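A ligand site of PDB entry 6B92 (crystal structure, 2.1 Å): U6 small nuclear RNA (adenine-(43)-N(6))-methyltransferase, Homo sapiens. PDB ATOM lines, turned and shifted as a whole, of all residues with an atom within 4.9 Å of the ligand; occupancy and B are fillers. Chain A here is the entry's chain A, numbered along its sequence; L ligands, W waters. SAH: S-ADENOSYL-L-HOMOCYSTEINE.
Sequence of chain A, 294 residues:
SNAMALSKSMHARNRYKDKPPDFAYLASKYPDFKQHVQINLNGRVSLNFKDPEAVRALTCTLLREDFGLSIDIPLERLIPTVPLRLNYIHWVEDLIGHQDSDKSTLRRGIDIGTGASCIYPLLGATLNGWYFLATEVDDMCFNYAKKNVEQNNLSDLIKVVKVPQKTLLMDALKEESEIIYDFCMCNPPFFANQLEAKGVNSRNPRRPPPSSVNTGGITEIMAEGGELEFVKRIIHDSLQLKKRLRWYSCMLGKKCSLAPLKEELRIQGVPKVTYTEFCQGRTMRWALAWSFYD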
ATOM      1  N   LEU A  78       2.922  24.207  -5.180  1.00  0.00           N
ATOM      2  CA  LEU A  78       2.433  25.568  -5.460  1.00  0.00           C
ATOM      3  C   LEU A  78       0.956  25.771  -5.021  1.00  0.00           C
ATOM      4  O   LEU A  78       0.073  24.971  -5.347  1.00  0.00           O
ATOM      5  CB  LEU A  78       2.584  25.924  -6.931  1.00  0.00           C
ATOM      6  CG  LEU A  78       2.123  27.333  -7.329  1.00  0.00           C
ATOM      7  CD1 LEU A  78       3.169  28.411  -6.991  1.00  0.00           C
ATOM      8  CD2 LEU A  78       1.752  27.357  -8.802  1.00  0.00           C
ATOM      9  N   PRO A  80      -2.077  28.254  -5.541  1.00  0.00           N
ATOM     10  CA  PRO A  80      -2.483  29.299  -6.458  1.00  0.00           C
ATOM     11  C   PRO A  80      -3.213  30.457  -5.784  1.00  0.00           C
ATOM     12  O   PRO A  80      -3.864  30.300  -4.718  1.00  0.00           O
ATOM     13  CB  PRO A  80      -3.435  28.571  -7.408  1.00  0.00           C
ATOM     14  CG  PRO A  80      -4.027  27.486  -6.575  1.00  0.00           C
ATOM     15  CD  PRO A  80      -2.947  27.050  -5.634  1.00  0.00           C
ATOM     16  N   ARG A  85      -5.877  33.692 -11.202  1.00  0.00           N
ATOM     17  CA  ARG A  85      -6.258  32.588 -12.127  1.00  0.00           C
ATOM     18  C   ARG A  85      -7.542  32.879 -12.917  1.00  0.00           C
ATOM     19  O   ARG A  85      -7.633  32.478 -14.077  1.00  0.00           O
ATOM     20  CB  ARG A  85      -6.445  31.269 -11.353  1.00  0.00           C
ATOM     21  CG  ARG A  85      -5.225  30.760 -10.596  1.00  0.00           C
ATOM     22  CD  ARG A  85      -3.942  30.948 -11.378  1.00  0.00           C
ATOM     23  NE  ARG A  85      -2.814  30.337 -10.699  1.00  0.00           N
ATOM     24  CZ  ARG A  85      -2.458  29.060 -10.830  1.00  0.00           C
ATOM     25  NH1 ARG A  85      -3.164  28.240 -11.638  1.00  0.00           N
ATOM     26  NH2 ARG A  85      -1.403  28.602 -10.184  1.00  0.00           N
ATOM     27  N   ASP A 111      -5.392  21.453 -19.735  1.00  0.00           N
ATOM     28  CA  ASP A 111      -4.583  22.197 -18.792  1.00  0.00           C
ATOM     29  C   ASP A 111      -3.292  21.405 -18.594  1.00  0.00           C
ATOM     30  O   ASP A 111      -3.309  20.295 -18.077  1.00  0.00           O
ATOM     31  CB  ASP A 111      -5.323  22.403 -17.453  1.00  0.00           C
ATOM     32  CG  ASP A 111      -4.512  23.240 -16.432  1.00  0.00           C
ATOM     33  OD1 ASP A 111      -3.635  24.035 -16.842  1.00  0.00           O
ATOM     34  OD2 ASP A 111      -4.759  23.108 -15.209  1.00  0.00           O
ATOM     35  N   ILE A 112      -2.190  21.990 -19.014  1.00  0.00           N
ATOM     36  CA  ILE A 112      -0.878  21.365 -18.968  1.00  0.00           C
ATOM     37  C   ILE A 112      -0.221  21.675 -17.640  1.00  0.00           C
ATOM     38  O   ILE A 112       0.102  22.820 -17.408  1.00  0.00           O
ATOM     39  CB  ILE A 112       0.073  21.902 -20.068  1.00  0.00           C
ATOM     40  CG1 ILE A 112      -0.477  21.590 -21.454  1.00  0.00           C
ATOM     41  CG2 ILE A 112       1.470  21.309 -19.913  1.00  0.00           C
ATOM     42  CD1 ILE A 112      -0.017  22.594 -22.481  1.00  0.00           C
ATOM     43  N   GLY A 113      -0.043  20.656 -16.790  1.00  0.00           N
ATOM     44  CA  GLY A 113       0.550  20.828 -15.487  1.00  0.00           C
ATOM     45  C   GLY A 113      -0.457  21.427 -14.540  1.00  0.00           C
ATOM     46  O   GLY A 113      -0.306  22.552 -14.106  1.00  0.00           O
ATOM     47  N   THR A 114      -1.497  20.663 -14.230  1.00  0.00           N
ATOM     48  CA  THR A 114      -2.678  21.194 -13.574  1.00  0.00           C
ATOM     49  C   THR A 114      -2.444  21.558 -12.125  1.00  0.00           C
ATOM     50  O   THR A 114      -3.134  22.394 -11.600  1.00  0.00           O
ATOM     51  CB  THR A 114      -3.890  20.276 -13.754  1.00  0.00           C
ATOM     52  OG1 THR A 114      -5.080  21.022 -13.556  1.00  0.00           O
ATOM     53  CG2 THR A 114      -3.856  19.085 -12.816  1.00  0.00           C
ATOM     54  N   GLY A 115      -1.436  20.964 -11.481  1.00  0.00           N
ATOM     55  CA  GLY A 115      -1.101  21.296 -10.091  1.00  0.00           C
ATOM     56  C   GLY A 115      -2.024  20.597  -9.094  1.00  0.00           C
ATOM     57  O   GLY A 115      -3.046  20.003  -9.451  1.00  0.00           O
ATOM     58  N   ALA A 116      -1.648  20.667  -7.834  1.00  0.00           N
ATOM     59  CA  ALA A 116      -2.367  19.980  -6.773  1.00  0.00           C
ATOM     60  C   ALA A 116      -3.802  20.480  -6.609  1.00  0.00           C
ATOM     61  O   ALA A 116      -4.685  19.690  -6.320  1.00  0.00           O
ATOM     62  CB  ALA A 116      -1.585  20.081  -5.466  1.00  0.00           C
ATOM     63  N   SER A 117      -4.040  21.744  -6.877  1.00  0.00           N
ATOM     64  CA  SER A 117      -5.373  22.383  -6.754  1.00  0.00           C
ATOM     65  C   SER A 117      -6.279  22.074  -7.940  1.00  0.00           C
ATOM     66  O   SER A 117      -7.500  22.250  -7.854  1.00  0.00           O
ATOM     67  CB  SER A 117      -5.158  23.894  -6.694  1.00  0.00           C
ATOM     68  OG  SER A 117      -4.627  24.313  -8.001  1.00  0.00           O
ATOM     69  N   ILE A 119      -6.754  23.853 -10.412  1.00  0.00           N
ATOM     70  CA  ILE A 119      -7.574  25.034 -10.303  1.00  0.00           C
ATOM     71  C   ILE A 119      -8.184  25.543 -11.614  1.00  0.00           C
ATOM     72  O   ILE A 119      -9.357  25.932 -11.608  1.00  0.00           O
ATOM     73  CB  ILE A 119      -6.873  26.143  -9.533  1.00  0.00           C
ATOM     74  CG1 ILE A 119      -7.956  27.149  -9.087  1.00  0.00           C
ATOM     75  CG2 ILE A 119      -5.708  26.722 -10.327  1.00  0.00           C
ATOM     76  CD1 ILE A 119      -7.412  28.409  -8.489  1.00  0.00           C
ATOM     77  N   TYR A 120      -7.457  25.514 -12.737  1.00  0.00           N
ATOM     78  CA  TYR A 120      -8.064  25.996 -13.967  1.00  0.00           C
ATOM     79  C   TYR A 120      -9.234  25.115 -14.364  1.00  0.00           C
ATOM     80  O   TYR A 120     -10.311  25.635 -14.612  1.00  0.00           O
ATOM     81  CB  TYR A 120      -7.084  26.203 -15.117  1.00  0.00           C
ATOM     82  CG  TYR A 120      -6.050  27.294 -14.952  1.00  0.00           C
ATOM     83  CD1 TYR A 120      -6.396  28.610 -14.589  1.00  0.00           C
ATOM     84  CD2 TYR A 120      -4.696  27.014 -15.221  1.00  0.00           C
ATOM     85  CE1 TYR A 120      -5.404  29.614 -14.507  1.00  0.00           C
ATOM     86  CE2 TYR A 120      -3.727  27.997 -15.101  1.00  0.00           C
ATOM     87  CZ  TYR A 120      -4.077  29.281 -14.759  1.00  0.00           C
ATOM     88  OH  TYR A 120      -3.041  30.200 -14.640  1.00  0.00           O
ATOM     89  N   THR A 135      -3.246  17.495 -17.220  1.00  0.00           N
ATOM     90  CA  THR A 135      -2.055  16.648 -17.153  1.00  0.00           C
ATOM     91  C   THR A 135      -1.155  17.076 -16.021  1.00  0.00           C
ATOM     92  O   THR A 135      -1.156  18.255 -15.636  1.00  0.00           O
ATOM     93  CB  THR A 135      -1.223  16.674 -18.446  1.00  0.00           C
ATOM     94  OG1 THR A 135      -0.614  17.954 -18.617  1.00  0.00           O
ATOM     95  CG2 THR A 135      -2.073  16.339 -19.655  1.00  0.00           C
ATOM     96  N   GLU A 136      -0.430  16.099 -15.481  1.00  0.00           N
ATOM     97  CA  GLU A 136       0.596  16.324 -14.471  1.00  0.00           C
ATOM     98  C   GLU A 136       1.706  15.282 -14.591  1.00  0.00           C
ATOM     99  O   GLU A 136       1.439  14.101 -14.836  1.00  0.00           O
ATOM    100  CB  GLU A 136       0.032  16.198 -13.044  1.00  0.00           C
ATOM    101  CG  GLU A 136      -0.079  17.481 -12.230  1.00  0.00           C
ATOM    102  CD  GLU A 136       1.186  18.320 -12.173  1.00  0.00           C
ATOM    103  OE1 GLU A 136       0.991  19.560 -12.094  1.00  0.00           O
ATOM    104  OE2 GLU A 136       2.334  17.758 -12.168  1.00  0.00           O
ATOM    105  N   VAL A 137       2.953  15.711 -14.375  1.00  0.00           N
ATOM    106  CA  VAL A 137       4.092  14.782 -14.222  1.00  0.00           C
ATOM    107  C   VAL A 137       4.406  14.450 -12.778  1.00  0.00           C
ATOM    108  O   VAL A 137       4.996  13.420 -12.515  1.00  0.00           O
ATOM    109  CB  VAL A 137       5.394  15.277 -14.908  1.00  0.00           C
ATOM    110  CG1 VAL A 137       5.162  15.444 -16.399  1.00  0.00           C
ATOM    111  CG2 VAL A 137       5.923  16.575 -14.303  1.00  0.00           C
ATOM    112  N   ASP A 138       4.069  15.353 -11.861  1.00  0.00           N
ATOM    113  CA  ASP A 138       4.392  15.182 -10.450  1.00  0.00           C
ATOM    114  C   ASP A 138       3.364  14.281  -9.773  1.00  0.00           C
ATOM    115  O   ASP A 138       2.147  14.479  -9.919  1.00  0.00           O
ATOM    116  CB  ASP A 138       4.450  16.518  -9.750  1.00  0.00           C
ATOM    117  CG  ASP A 138       4.871  16.386  -8.348  1.00  0.00           C
ATOM    118  OD1 ASP A 138       6.049  15.995  -8.132  1.00  0.00           O
ATOM    119  OD2 ASP A 138       4.027  16.617  -7.445  1.00  0.00           O
ATOM    120  N   CYS A 141       1.105  16.120  -6.926  1.00  0.00           N
ATOM    121  CA  CYS A 141       0.146  17.020  -7.562  1.00  0.00           C
ATOM    122  C   CYS A 141      -0.928  16.218  -8.262  1.00  0.00           C
ATOM    123  O   CYS A 141      -2.077  16.563  -8.161  1.00  0.00           O
ATOM    124  CB  CYS A 141       0.822  17.966  -8.572  1.00  0.00           C
ATOM    125  SG  CYS A 141       1.836  19.303  -7.912  1.00  0.00           S
ATOM    126  N   VAL A 163       1.254  11.925 -16.801  1.00  0.00           N
ATOM    127  CA  VAL A 163       1.982  11.722 -18.041  1.00  0.00           C
ATOM    128  C   VAL A 163       3.459  11.554 -17.715  1.00  0.00           C
ATOM    129  O   VAL A 163       3.910  11.997 -16.646  1.00  0.00           O
ATOM    130  CB  VAL A 163       1.825  12.889 -19.033  1.00  0.00           C
ATOM    131  CG1 VAL A 163       0.374  13.066 -19.417  1.00  0.00           C
ATOM    132  CG2 VAL A 163       2.453  14.175 -18.486  1.00  0.00           C
ATOM    133  N   GLN A 165       7.438  12.166 -17.580  1.00  0.00           N
ATOM    134  CA  GLN A 165       8.374  13.296 -17.477  1.00  0.00           C
ATOM    135  C   GLN A 165       8.741  14.092 -18.742  1.00  0.00           C
ATOM    136  O   GLN A 165       8.876  15.323 -18.704  1.00  0.00           O
ATOM    137  CB  GLN A 165       9.703  12.795 -16.798  1.00  0.00           C
ATOM    138  CG  GLN A 165       9.841  13.171 -15.321  1.00  0.00           C
ATOM    139  CD  GLN A 165       9.844  14.687 -15.093  1.00  0.00           C
ATOM    140  OE1 GLN A 165      10.336  15.470 -15.931  1.00  0.00           O
ATOM    141  NE2 GLN A 165       9.269  15.122 -13.972  1.00  0.00           N
ATOM    142  N   THR A 167       7.108  14.346 -21.686  1.00  0.00           N
ATOM    143  CA  THR A 167       6.041  14.490 -22.659  1.00  0.00           C
ATOM    144  C   THR A 167       5.270  15.760 -22.435  1.00  0.00           C
ATOM    145  O   THR A 167       5.358  16.408 -21.383  1.00  0.00           O
ATOM    146  CB  THR A 167       5.076  13.314 -22.563  1.00  0.00           C
ATOM    147  OG1 THR A 167       4.541  13.237 -21.253  1.00  0.00           O
ATOM    148  CG2 THR A 167       5.834  11.960 -22.866  1.00  0.00           C
ATOM    149  N   LEU A 168       4.506  16.144 -23.439  1.00  0.00           N
ATOM    150  CA  LEU A 168       3.728  17.348 -23.356  1.00  0.00           C
ATOM    151  C   LEU A 168       2.386  17.074 -24.039  1.00  0.00           C
ATOM    152  O   LEU A 168       1.717  16.128 -23.631  1.00  0.00           O
ATOM    153  CB  LEU A 168       4.545  18.513 -23.932  1.00  0.00           C
ATOM    154  CG  LEU A 168       4.096  19.937 -23.645  1.00  0.00           C
ATOM    155  CD1 LEU A 168       4.112  20.211 -22.159  1.00  0.00           C
ATOM    156  CD2 LEU A 168       5.055  20.922 -24.322  1.00  0.00           C
ATOM    157  N   ASN A 187       0.408  27.675 -17.112  1.00  0.00           N
ATOM    158  CA  ASN A 187       1.054  28.846 -16.450  1.00  0.00           C
ATOM    159  C   ASN A 187       2.358  28.422 -15.795  1.00  0.00           C
ATOM    160  O   ASN A 187       2.715  27.246 -15.938  1.00  0.00           O
ATOM    161  CB  ASN A 187       0.057  29.536 -15.494  1.00  0.00           C
ATOM    162  CG  ASN A 187      -0.098  28.802 -14.196  1.00  0.00           C
ATOM    163  OD1 ASN A 187      -0.237  27.582 -14.204  1.00  0.00           O
ATOM    164  ND2 ASN A 187      -0.105  29.523 -13.075  1.00  0.00           N
ATOM    165  N   PRO A 188       3.097  29.371 -15.127  1.00  0.00           N
ATOM    166  CA  PRO A 188       4.337  29.055 -14.372  1.00  0.00           C
ATOM    167  C   PRO A 188       4.077  28.374 -12.987  1.00  0.00           C
ATOM    168  O   PRO A 188       2.893  28.375 -12.540  1.00  0.00           O
ATOM    169  CB  PRO A 188       4.990  30.463 -14.158  1.00  0.00           C
ATOM    170  CG  PRO A 188       4.099  31.478 -14.868  1.00  0.00           C
ATOM    171  CD  PRO A 188       2.751  30.811 -14.969  1.00  0.00           C
ATOM    172  N   PRO A 189       5.106  27.814 -12.291  1.00  0.00           N
ATOM    173  CA  PRO A 189       6.553  27.850 -12.687  1.00  0.00           C
ATOM    174  C   PRO A 189       6.991  26.801 -13.740  1.00  0.00           C
ATOM    175  O   PRO A 189       6.374  25.742 -13.868  1.00  0.00           O
ATOM    176  CB  PRO A 189       7.278  27.585 -11.349  1.00  0.00           C
ATOM    177  CG  PRO A 189       6.321  26.755 -10.554  1.00  0.00           C
ATOM    178  CD  PRO A 189       4.909  27.054 -11.037  1.00  0.00           C
ATOM    179  N   PHE A 230      10.217  26.006 -22.018  1.00  0.00           N
ATOM    180  CA  PHE A 230       9.020  25.222 -21.826  1.00  0.00           C
ATOM    181  C   PHE A 230       7.983  25.620 -22.842  1.00  0.00           C
ATOM    182  O   PHE A 230       7.406  24.767 -23.503  1.00  0.00           O
ATOM    183  CB  PHE A 230       8.460  25.397 -20.435  1.00  0.00           C
ATOM    184  CG  PHE A 230       7.356  24.456 -20.119  1.00  0.00           C
ATOM    185  CD1 PHE A 230       6.053  24.782 -20.428  1.00  0.00           C
ATOM    186  CD2 PHE A 230       7.630  23.225 -19.565  1.00  0.00           C
ATOM    187  CE1 PHE A 230       5.020  23.906 -20.165  1.00  0.00           C
ATOM    188  CE2 PHE A 230       6.597  22.330 -19.292  1.00  0.00           C
ATOM    189  CZ  PHE A 230       5.291  22.675 -19.592  1.00  0.00           C
ATOM    190  N   ARG A 233       8.578  24.141 -26.324  1.00  0.00           N
ATOM    191  CA  ARG A 233       8.015  22.787 -26.398  1.00  0.00           C
ATOM    192  C   ARG A 233       6.527  22.820 -26.773  1.00  0.00           C
ATOM    193  O   ARG A 233       6.082  22.035 -27.591  1.00  0.00           O
ATOM    194  CB  ARG A 233       8.220  21.997 -25.097  1.00  0.00           C
ATOM    195  CG  ARG A 233       9.697  21.729 -24.769  1.00  0.00           C
ATOM    196  CD  ARG A 233       9.906  21.175 -23.352  1.00  0.00           C
ATOM    197  NE  ARG A 233       9.201  19.897 -23.143  1.00  0.00           N
ATOM    198  CZ  ARG A 233       8.957  19.362 -21.940  1.00  0.00           C
ATOM    199  NH1 ARG A 233       9.353  19.991 -20.821  1.00  0.00           N
ATOM    200  NH2 ARG A 233       8.306  18.206 -21.858  1.00  0.00           N
HETATM  201  N   SAH L   1      -1.490  25.405 -13.171  1.00  0.00           N
HETATM  202  CA  SAH L   1      -0.444  24.876 -12.202  1.00  0.00           C
HETATM  203  CB  SAH L   1       1.032  25.414 -12.405  1.00  0.00           C
HETATM  204  CG  SAH L   1       1.567  24.986 -13.794  1.00  0.00           C
HETATM  205  SD  SAH L   1       3.402  25.011 -13.853  1.00  0.00           S
HETATM  206  C   SAH L   1      -0.818  25.212 -10.722  1.00  0.00           C
HETATM  207  O   SAH L   1      -0.268  24.624  -9.789  1.00  0.00           O
HETATM  208  OXT SAH L   1      -1.661  26.054 -10.457  1.00  0.00           O
HETATM  209  C5' SAH L   1       3.956  23.770 -12.643  1.00  0.00           C
HETATM  210  C4' SAH L   1       3.285  22.444 -12.770  1.00  0.00           C
HETATM  211  O4' SAH L   1       3.559  21.864 -14.044  1.00  0.00           O
HETATM  212  C3' SAH L   1       3.873  21.493 -11.673  1.00  0.00           C
HETATM  213  O3' SAH L   1       2.751  20.964 -11.026  1.00  0.00           O
HETATM  214  C2' SAH L   1       4.644  20.423 -12.516  1.00  0.00           C
HETATM  215  O2' SAH L   1       4.509  19.142 -11.978  1.00  0.00           O
HETATM  216  C1' SAH L   1       3.821  20.477 -13.871  1.00  0.00           C
HETATM  217  N9  SAH L   1       4.562  20.096 -15.065  1.00  0.00           N
HETATM  218  C8  SAH L   1       5.908  20.434 -15.461  1.00  0.00           C
HETATM  219  N7  SAH L   1       6.217  19.911 -16.652  1.00  0.00           N
HETATM  220  C5  SAH L   1       5.061  19.221 -17.082  1.00  0.00           C
HETATM  221  C6  SAH L   1       4.747  18.456 -18.269  1.00  0.00           C
HETATM  222  N6  SAH L   1       5.663  18.290 -19.236  1.00  0.00           N
HETATM  223  N1  SAH L   1       3.491  17.856 -18.431  1.00  0.00           N
HETATM  224  C2  SAH L   1       2.606  18.047 -17.400  1.00  0.00           C
HETATM  225  N3  SAH L   1       2.777  18.747 -16.228  1.00  0.00           N
HETATM  226  C4  SAH L   1       4.019  19.334 -16.108  1.00  0.00           C
HETATM  227  O   HOH W   1       1.418  17.389 -20.332  1.00  0.00           O
HETATM  228  O   HOH W   2      -4.421  24.386 -12.903  1.00  0.00           O
HETATM  229  O   HOH W   3       0.377  22.664  -7.222  1.00  0.00           O
HETATM  230  O   HOH W   4      -2.059  24.336  -7.835  1.00  0.00           O
HETATM  231  O   HOH W   5       8.671  18.213 -18.583  1.00  0.00           O
HETATM  232  O   HOH W   6       2.139  23.098  -9.495  1.00  0.00           O
HETATM  233  O   HOH W   7      -1.341  24.962 -15.953  1.00  0.00           O
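A nitrogen (N6) of the ligand sits at hydrogen-bond distance from the backbone carbonyl oxygen of Thr 167, 2.9 Å away.
OE1 of Glu 136 lies within hydrogen-bond range of O3' of the ligand (2.5 Å).
SG of Cys 141 is in hydrogen-bond range of O3' of the ligand (3.6 Å).
The side-chain amide oxygen (OD1) of Asn 187 lies within hydrogen-bond range of a nitrogen (N) of the ligand, 2.7 Å away.
The backbone carbonyl oxygen (O) of Gly 113 lies close to a nitrogen (N) of the ligand (3.2 Å).
NH2 of Arg 85 is in salt-bridge range of OXT of the ligand.
N of Gly 113 sits close to N3 of the ligand.
The backbone NH (N) of Cys 141 lies within hydrogen-bond range of the side-chain carboxylate (OD2) of Asp 138, at 3.0 Å.
The guanidinium group (NH2) of Arg 85 sits close to the side-chain amide nitrogen (ND2) of Asn 187 (3.3 Å).
The backbone carbonyl oxygen of Glu 136 sits at hydrogen-bond distance from the backbone NH of Val 163 (2.9 Å).
The side-chain carboxylate (OD2) of Asp 111 sits at hydrogen-bond distance from the side-chain hydroxyl (OG1) of Thr 114 (2.7 Å).
OE1 of Glu 136 lies within hydrogen-bond range of N of Gly 115, 2.9 Å away.
OE1 of Glu 136 sits at hydrogen-bond distance from N of Thr 114.
OE2 of Glu 136 is in hydrogen-bond range of N of Asp 138, at 3.0 Å.
O of Thr 135 is in hydrogen-bond range of N of Thr 114 (2.8 Å).
O of Pro 188 lies close to SD of the ligand, 3.6 Å away.
O of Pro 189 sits close to SD of the ligand, 3.1 Å away.
Residues that only touch the ligand: Leu 78, Thr 114, Gly 115, Tyr 120, Thr 135, Val 137, Asp 138, Val 163, Leu 168, Phe 230 and Arg 233.
Hydrophobic or aromatic side chains within 4 Å of the ligand: Leu 78, Tyr 120, Val 137, Val 163, Leu 168, Pro 189 and Phe 230.
Along chain A the residues within 4 Å of the ligand span positions 78 to 233.
The nearest printed residue that does not touch the ligand is Ile 119 (4.1 Å).
Water W4 lies within hydrogen-bond range of the side-chain hydroxyl of Ser 117, an oxygen (O) of the ligand and the backbone carbonyl oxygen of Leu 78.
Water W1 lies within hydrogen-bond range of OG1 of Thr 135 (2.7 Å) and N1 of the ligand (2.9 Å).
Water W5 lies within hydrogen-bond range of O of Gln 165 (2.9 Å), NH1 of Arg 233 (2.9 Å) and N6 of the ligand (3.1 Å).
Water W2 lies within hydrogen-bond range of the side-chain carboxylate (OD2) of Asp 111, the backbone carbonyl oxygen (O) of Thr 114, a nitrogen (N) of the ligand, the backbone NH (N) of Tyr 120 and the backbone NH (N) of Ile 119.
Water W3 lies within hydrogen-bond range of the backbone NH (N) of Ala 116 (2.9 Å), the backbone carbonyl oxygen (O) of Leu 78 (3.0 Å), an oxygen (O) of the ligand (3.3 Å) and the side-chain sulfur (SG) of Cys 141 (3.7 Å).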
